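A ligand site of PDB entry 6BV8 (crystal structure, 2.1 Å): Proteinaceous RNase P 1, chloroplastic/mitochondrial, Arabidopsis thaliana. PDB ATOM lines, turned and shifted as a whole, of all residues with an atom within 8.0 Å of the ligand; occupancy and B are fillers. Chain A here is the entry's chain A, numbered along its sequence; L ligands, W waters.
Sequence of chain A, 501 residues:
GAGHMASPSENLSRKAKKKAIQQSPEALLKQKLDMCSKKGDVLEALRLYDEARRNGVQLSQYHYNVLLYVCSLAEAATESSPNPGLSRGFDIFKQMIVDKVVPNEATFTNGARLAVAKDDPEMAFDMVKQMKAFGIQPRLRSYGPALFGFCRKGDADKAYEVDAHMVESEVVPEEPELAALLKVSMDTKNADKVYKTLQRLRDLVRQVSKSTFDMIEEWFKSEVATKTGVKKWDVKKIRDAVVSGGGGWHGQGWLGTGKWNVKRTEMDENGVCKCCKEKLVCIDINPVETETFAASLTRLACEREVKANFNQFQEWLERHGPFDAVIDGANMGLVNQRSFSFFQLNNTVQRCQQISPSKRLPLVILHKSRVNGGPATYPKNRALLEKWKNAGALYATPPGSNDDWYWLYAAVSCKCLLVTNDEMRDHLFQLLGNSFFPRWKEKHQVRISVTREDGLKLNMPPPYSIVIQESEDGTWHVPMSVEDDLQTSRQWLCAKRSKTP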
ATOM      1  N   ASN A 270       5.642 -21.028  24.081  1.00  0.00           N
ATOM      2  CA  ASN A 270       4.171 -21.000  24.030  1.00  0.00           C
ATOM      3  C   ASN A 270       3.567 -20.153  22.904  1.00  0.00           C
ATOM      4  O   ASN A 270       2.341 -19.980  22.880  1.00  0.00           O
ATOM      5  CB  ASN A 270       3.633 -20.508  25.364  1.00  0.00           C
ATOM      6  CG  ASN A 270       4.108 -21.370  26.507  1.00  0.00           C
ATOM      7  OD1 ASN A 270       4.090 -22.596  26.422  1.00  0.00           O
ATOM      8  ND2 ASN A 270       4.555 -20.733  27.575  1.00  0.00           N
ATOM      9  N   LYS A 279       0.002 -13.537  21.986  1.00  0.00           N
ATOM     10  CA  LYS A 279       0.005 -14.998  21.901  1.00  0.00           C
ATOM     11  C   LYS A 279      -0.513 -15.376  20.526  1.00  0.00           C
ATOM     12  O   LYS A 279      -1.645 -15.105  20.198  1.00  0.00           O
ATOM     13  CB  LYS A 279      -0.877 -15.627  22.979  1.00  0.00           C
ATOM     14  CG  LYS A 279      -0.618 -17.120  23.160  1.00  0.00           C
ATOM     15  CD  LYS A 279      -1.632 -17.741  24.106  1.00  0.00           C
ATOM     16  CE  LYS A 279      -1.678 -19.256  23.996  1.00  0.00           C
ATOM     17  NZ  LYS A 279      -0.382 -19.893  24.381  1.00  0.00           N
ATOM     18  N   LEU A 280       0.344 -16.014  19.737  1.00  0.00           N
ATOM     19  CA  LEU A 280      -0.032 -16.448  18.407  1.00  0.00           C
ATOM     20  C   LEU A 280      -1.085 -17.532  18.524  1.00  0.00           C
ATOM     21  O   LEU A 280      -1.170 -18.196  19.555  1.00  0.00           O
ATOM     22  CB  LEU A 280       1.194 -16.956  17.637  1.00  0.00           C
ATOM     23  CG  LEU A 280       2.275 -15.925  17.289  1.00  0.00           C
ATOM     24  CD1 LEU A 280       3.158 -16.517  16.212  1.00  0.00           C
ATOM     25  CD2 LEU A 280       1.715 -14.601  16.806  1.00  0.00           C
ATOM     26  N   VAL A 281      -1.887 -17.711  17.493  1.00  0.00           N
ATOM     27  CA  VAL A 281      -2.929 -18.721  17.545  1.00  0.00           C
ATOM     28  C   VAL A 281      -2.433 -20.033  16.990  1.00  0.00           C
ATOM     29  O   VAL A 281      -1.452 -20.103  16.208  1.00  0.00           O
ATOM     30  CB  VAL A 281      -4.213 -18.282  16.803  1.00  0.00           C
ATOM     31  CG1 VAL A 281      -4.627 -16.886  17.226  1.00  0.00           C
ATOM     32  CG2 VAL A 281      -4.061 -18.360  15.296  1.00  0.00           C
ATOM     33  N   CYS A 282      -3.145 -21.086  17.390  1.00  0.00           N
ATOM     34  CA  CYS A 282      -2.964 -22.397  16.867  1.00  0.00           C
ATOM     35  C   CYS A 282      -4.131 -22.687  15.950  1.00  0.00           C
ATOM     36  O   CYS A 282      -5.269 -22.629  16.359  1.00  0.00           O
ATOM     37  CB  CYS A 282      -2.944 -23.435  17.993  1.00  0.00           C
ATOM     38  SG  CYS A 282      -2.298 -24.987  17.334  1.00  0.00           S
ATOM     39  N   ILE A 283      -3.833 -23.054  14.711  1.00  0.00           N
ATOM     40  CA  ILE A 283      -4.865 -23.177  13.679  1.00  0.00           C
ATOM     41  C   ILE A 283      -5.149 -24.646  13.438  1.00  0.00           C
ATOM     42  O   ILE A 283      -4.220 -25.411  13.208  1.00  0.00           O
ATOM     43  CB  ILE A 283      -4.408 -22.540  12.349  1.00  0.00           C
ATOM     44  CG1 ILE A 283      -4.163 -21.042  12.548  1.00  0.00           C
ATOM     45  CG2 ILE A 283      -5.438 -22.789  11.238  1.00  0.00           C
ATOM     46  CD1 ILE A 283      -3.576 -20.359  11.328  1.00  0.00           C
ATOM     47  N   ASP A 284      -6.427 -25.011  13.428  1.00  0.00           N
ATOM     48  CA  ASP A 284      -6.862 -26.396  13.299  1.00  0.00           C
ATOM     49  C   ASP A 284      -6.691 -26.906  11.895  1.00  0.00           C
ATOM     50  O   ASP A 284      -6.661 -26.132  10.945  1.00  0.00           O
ATOM     51  CB  ASP A 284      -8.336 -26.539  13.676  1.00  0.00           C
ATOM     52  CG  ASP A 284      -8.604 -26.226  15.135  1.00  0.00           C
ATOM     53  OD1 ASP A 284      -7.653 -26.180  15.942  1.00  0.00           O
ATOM     54  OD2 ASP A 284      -9.784 -26.037  15.468  1.00  0.00           O
ATOM     55  N   ILE A 285      -6.599 -28.223  11.797  1.00  0.00           N
ATOM     56  CA  ILE A 285      -6.609 -28.934  10.537  1.00  0.00           C
ATOM     57  C   ILE A 285      -7.978 -29.613  10.407  1.00  0.00           C
ATOM     58  O   ILE A 285      -8.416 -30.353  11.279  1.00  0.00           O
ATOM     59  CB  ILE A 285      -5.471 -29.983  10.481  1.00  0.00           C
ATOM     60  CG1 ILE A 285      -4.119 -29.270  10.329  1.00  0.00           C
ATOM     61  CG2 ILE A 285      -5.712 -30.983   9.347  1.00  0.00           C
ATOM     62  CD1 ILE A 285      -2.930 -30.185  10.302  1.00  0.00           C
ATOM     63  N   LEU A 417       1.495 -39.132  16.984  1.00  0.00           N
ATOM     64  CA  LEU A 417       2.803 -38.490  16.834  1.00  0.00           C
ATOM     65  C   LEU A 417       3.668 -39.274  15.891  1.00  0.00           C
ATOM     66  O   LEU A 417       3.571 -40.486  15.814  1.00  0.00           O
ATOM     67  CB  LEU A 417       3.487 -38.354  18.176  1.00  0.00           C
ATOM     68  CG  LEU A 417       2.704 -37.508  19.168  1.00  0.00           C
ATOM     69  CD1 LEU A 417       3.295 -37.717  20.556  1.00  0.00           C
ATOM     70  CD2 LEU A 417       2.706 -36.029  18.800  1.00  0.00           C
ATOM     71  N   ARG A 439       1.544 -28.544   7.137  1.00  0.00           N
ATOM     72  CA  ARG A 439       0.689 -28.291   8.293  1.00  0.00           C
ATOM     73  C   ARG A 439       0.525 -29.536   9.176  1.00  0.00           C
ATOM     74  O   ARG A 439       0.550 -29.417  10.398  1.00  0.00           O
ATOM     75  CB  ARG A 439      -0.684 -27.721   7.880  1.00  0.00           C
ATOM     76  CG  ARG A 439      -0.601 -26.281   7.358  1.00  0.00           C
ATOM     77  CD  ARG A 439      -1.974 -25.733   7.014  1.00  0.00           C
ATOM     78  NE  ARG A 439      -2.485 -26.354   5.790  1.00  0.00           N
ATOM     79  CZ  ARG A 439      -3.662 -26.958   5.630  1.00  0.00           C
ATOM     80  NH1 ARG A 439      -4.554 -27.053   6.597  1.00  0.00           N
ATOM     81  NH2 ARG A 439      -3.966 -27.470   4.441  1.00  0.00           N
ATOM     82  N   TRP A 440       0.364 -30.713   8.547  1.00  0.00           N
ATOM     83  CA  TRP A 440       0.182 -31.976   9.270  1.00  0.00           C
ATOM     84  C   TRP A 440       1.489 -32.277  10.024  1.00  0.00           C
ATOM     85  O   TRP A 440       1.446 -32.532  11.205  1.00  0.00           O
ATOM     86  CB  TRP A 440      -0.197 -33.139   8.309  1.00  0.00           C
ATOM     87  CG  TRP A 440      -0.374 -34.435   8.997  1.00  0.00           C
ATOM     88  CD1 TRP A 440      -1.519 -34.938   9.499  1.00  0.00           C
ATOM     89  CD2 TRP A 440       0.668 -35.382   9.311  1.00  0.00           C
ATOM     90  NE1 TRP A 440      -1.276 -36.148  10.131  1.00  0.00           N
ATOM     91  CE2 TRP A 440       0.049 -36.446  10.012  1.00  0.00           C
ATOM     92  CE3 TRP A 440       2.041 -35.424   9.094  1.00  0.00           C
ATOM     93  CZ2 TRP A 440       0.776 -37.545  10.469  1.00  0.00           C
ATOM     94  CZ3 TRP A 440       2.755 -36.523   9.526  1.00  0.00           C
ATOM     95  CH2 TRP A 440       2.127 -37.569  10.232  1.00  0.00           C
ATOM     96  N   GLU A 442       3.791 -30.303  11.138  1.00  0.00           N
ATOM     97  CA  GLU A 442       3.972 -29.400  12.258  1.00  0.00           C
ATOM     98  C   GLU A 442       3.208 -29.909  13.488  1.00  0.00           C
ATOM     99  O   GLU A 442       3.740 -29.915  14.615  1.00  0.00           O
ATOM    100  CB  GLU A 442       3.516 -28.004  11.870  1.00  0.00           C
ATOM    101  CG  GLU A 442       3.386 -27.014  13.016  1.00  0.00           C
ATOM    102  CD  GLU A 442       3.131 -25.596  12.520  1.00  0.00           C
ATOM    103  OE1 GLU A 442       1.978 -25.154  12.433  1.00  0.00           O
ATOM    104  OE2 GLU A 442       4.097 -24.912  12.187  1.00  0.00           O
ATOM    105  N   LYS A 443       1.965 -30.344  13.275  1.00  0.00           N
ATOM    106  CA  LYS A 443       1.181 -30.850  14.388  1.00  0.00           C
ATOM    107  C   LYS A 443       1.578 -32.222  14.863  1.00  0.00           C
ATOM    108  O   LYS A 443       1.249 -32.560  15.978  1.00  0.00           O
ATOM    109  CB  LYS A 443      -0.309 -30.833  14.045  1.00  0.00           C
ATOM    110  CG  LYS A 443      -0.842 -29.433  13.886  1.00  0.00           C
ATOM    111  CD  LYS A 443      -2.353 -29.434  13.901  1.00  0.00           C
ATOM    112  CE  LYS A 443      -2.893 -28.034  13.730  1.00  0.00           C
ATOM    113  NZ  LYS A 443      -2.614 -27.163  14.894  1.00  0.00           N
ATOM    114  N   HIS A 444       2.215 -33.042  14.025  1.00  0.00           N
ATOM    115  CA  HIS A 444       2.480 -34.472  14.350  1.00  0.00           C
ATOM    116  C   HIS A 444       3.937 -34.858  14.619  1.00  0.00           C
ATOM    117  O   HIS A 444       4.182 -35.791  15.343  1.00  0.00           O
ATOM    118  CB  HIS A 444       1.861 -35.390  13.291  1.00  0.00           C
ATOM    119  CG  HIS A 444       0.366 -35.306  13.247  1.00  0.00           C
ATOM    120  ND1 HIS A 444      -0.441 -36.243  13.866  1.00  0.00           N
ATOM    121  CD2 HIS A 444      -0.478 -34.381  12.736  1.00  0.00           C
ATOM    122  CE1 HIS A 444      -1.703 -35.899  13.719  1.00  0.00           C
ATOM    123  NE2 HIS A 444      -1.750 -34.761  13.048  1.00  0.00           N
ATOM    124  N   GLN A 445       4.884 -34.113  14.062  1.00  0.00           N
ATOM    125  CA  GLN A 445       6.275 -34.520  14.102  1.00  0.00           C
ATOM    126  C   GLN A 445       6.947 -34.224  15.435  1.00  0.00           C
ATOM    127  O   GLN A 445       6.923 -33.105  15.900  1.00  0.00           O
ATOM    128  CB  GLN A 445       7.093 -33.873  12.970  1.00  0.00           C
ATOM    129  CG  GLN A 445       8.571 -34.234  13.009  1.00  0.00           C
ATOM    130  CD  GLN A 445       9.363 -33.597  11.866  1.00  0.00           C
ATOM    131  OE1 GLN A 445       9.010 -32.539  11.385  1.00  0.00           O
ATOM    132  NE2 GLN A 445      10.415 -34.266  11.430  1.00  0.00           N
ATOM    133  N   MET A 460       8.539 -31.618  20.980  1.00  0.00           N
ATOM    134  CA  MET A 460       7.143 -31.843  20.664  1.00  0.00           C
ATOM    135  C   MET A 460       6.602 -30.806  19.674  1.00  0.00           C
ATOM    136  O   MET A 460       7.160 -29.727  19.528  1.00  0.00           O
ATOM    137  CB  MET A 460       6.327 -31.812  21.956  1.00  0.00           C
ATOM    138  CG  MET A 460       6.797 -32.803  23.016  1.00  0.00           C
ATOM    139  SD  MET A 460       6.780 -34.499  22.414  1.00  0.00           S
ATOM    140  CE  MET A 460       5.033 -34.838  22.396  1.00  0.00           C
ATOM    141  N   PRO A 461       5.469 -31.125  19.023  1.00  0.00           N
ATOM    142  CA  PRO A 461       4.777 -30.127  18.202  1.00  0.00           C
ATOM    143  C   PRO A 461       4.478 -28.813  18.967  1.00  0.00           C
ATOM    144  O   PRO A 461       4.110 -28.849  20.141  1.00  0.00           O
ATOM    145  CB  PRO A 461       3.487 -30.855  17.800  1.00  0.00           C
ATOM    146  CG  PRO A 461       3.892 -32.279  17.745  1.00  0.00           C
ATOM    147  CD  PRO A 461       4.784 -32.438  18.952  1.00  0.00           C
ATOM    148  N   PRO A 462       4.657 -27.657  18.318  1.00  0.00           N
ATOM    149  CA  PRO A 462       4.464 -26.429  19.048  1.00  0.00           C
ATOM    150  C   PRO A 462       2.973 -26.149  19.354  1.00  0.00           C
ATOM    151  O   PRO A 462       2.105 -26.624  18.633  1.00  0.00           O
ATOM    152  CB  PRO A 462       5.055 -25.373  18.100  1.00  0.00           C
ATOM    153  CG  PRO A 462       4.861 -25.928  16.751  1.00  0.00           C
ATOM    154  CD  PRO A 462       5.016 -27.421  16.905  1.00  0.00           C
ATOM    155  N   PRO A 463       2.680 -25.396  20.419  1.00  0.00           N
ATOM    156  CA  PRO A 463       1.286 -25.107  20.787  1.00  0.00           C
ATOM    157  C   PRO A 463       0.721 -23.883  20.056  1.00  0.00           C
ATOM    158  O   PRO A 463      -0.146 -23.212  20.574  1.00  0.00           O
ATOM    159  CB  PRO A 463       1.372 -24.848  22.301  1.00  0.00           C
ATOM    160  CG  PRO A 463       2.726 -24.291  22.497  1.00  0.00           C
ATOM    161  CD  PRO A 463       3.613 -24.978  21.468  1.00  0.00           C
ATOM    162  N   TYR A 464       1.238 -23.629  18.850  1.00  0.00           N
ATOM    163  CA  TYR A 464       0.778 -22.571  18.003  1.00  0.00           C
ATOM    164  C   TYR A 464       1.212 -22.918  16.594  1.00  0.00           C
ATOM    165  O   TYR A 464       2.055 -23.802  16.378  1.00  0.00           O
ATOM    166  CB  TYR A 464       1.341 -21.220  18.454  1.00  0.00           C
ATOM    167  CG  TYR A 464       2.837 -21.105  18.317  1.00  0.00           C
ATOM    168  CD1 TYR A 464       3.710 -21.742  19.224  1.00  0.00           C
ATOM    169  CD2 TYR A 464       3.397 -20.357  17.289  1.00  0.00           C
ATOM    170  CE1 TYR A 464       5.091 -21.651  19.081  1.00  0.00           C
ATOM    171  CE2 TYR A 464       4.774 -20.257  17.149  1.00  0.00           C
ATOM    172  CZ  TYR A 464       5.610 -20.911  18.050  1.00  0.00           C
ATOM    173  OH  TYR A 464       6.964 -20.776  17.874  1.00  0.00           O
ATOM    174  N   SER A 465       0.647 -22.227  15.621  1.00  0.00           N
ATOM    175  CA  SER A 465       0.991 -22.490  14.239  1.00  0.00           C
ATOM    176  C   SER A 465       2.068 -21.514  13.763  1.00  0.00           C
ATOM    177  O   SER A 465       1.939 -20.297  13.930  1.00  0.00           O
ATOM    178  CB  SER A 465      -0.253 -22.401  13.372  1.00  0.00           C
ATOM    179  OG  SER A 465      -1.253 -23.252  13.879  1.00  0.00           O
HETATM  180  O1  LIG L   1      -2.530 -25.865  22.176  1.00  0.00           O
HETATM  181  C1  LIG L   1      -2.182 -26.385  21.095  1.00  0.00           C
HETATM  182  C2  LIG L   1      -2.427 -25.680  19.907  1.00  0.00           C
HETATM  183  C3  LIG L   1      -2.051 -26.180  18.662  1.00  0.00           C
HETATM  184  C4  LIG L   1      -1.424 -27.412  18.482  1.00  0.00           C
HETATM  185  O2  LIG L   1      -1.120 -27.809  17.310  1.00  0.00           O
HETATM  186  C5  LIG L   1      -1.119 -28.232  19.689  1.00  0.00           C
HETATM  187  C6  LIG L   1      -1.513 -27.716  21.039  1.00  0.00           C
HETATM  188  C7  LIG L   1      -1.236 -28.483  22.184  1.00  0.00           C
HETATM  189  C8  LIG L   1      -0.594 -29.725  22.059  1.00  0.00           C
HETATM  190  C9  LIG L   1      -0.209 -30.243  20.808  1.00  0.00           C
HETATM  191  C10 LIG L   1      -0.451 -29.555  19.602  1.00  0.00           C
HETATM  192  O3  LIG L   1      -0.084 -30.038  18.363  1.00  0.00           O
HETATM  193  O   HOH W   1       2.927 -31.081  21.668  1.00  0.00           O
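Merely in contact with the ligand: Pro 463 (3.4 Å), Pro 462 (3.6 Å) and Pro 461 (3.7 Å). Of the 21 residues printed, 5 come within 4 Å of the ligand.
The side-chain sulfur (SG) of Cys 282 sits at hydrogen-bond distance from the side-chain amino group (NZ) of Lys 443 (3.3 Å). The backbone carbonyl oxygen of Ile 283 sits at hydrogen-bond distance from the side-chain amino group of Lys 443 (2.9 Å).
The side-chain amino group (NZ) of Lys 443 is in hydrogen-bond range of an oxygen (O2) of the ligand (2.9 Å). The side-chain sulfur of Cys 282 is covalently linked to a carbon (C3) of the ligand (1.8 Å).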
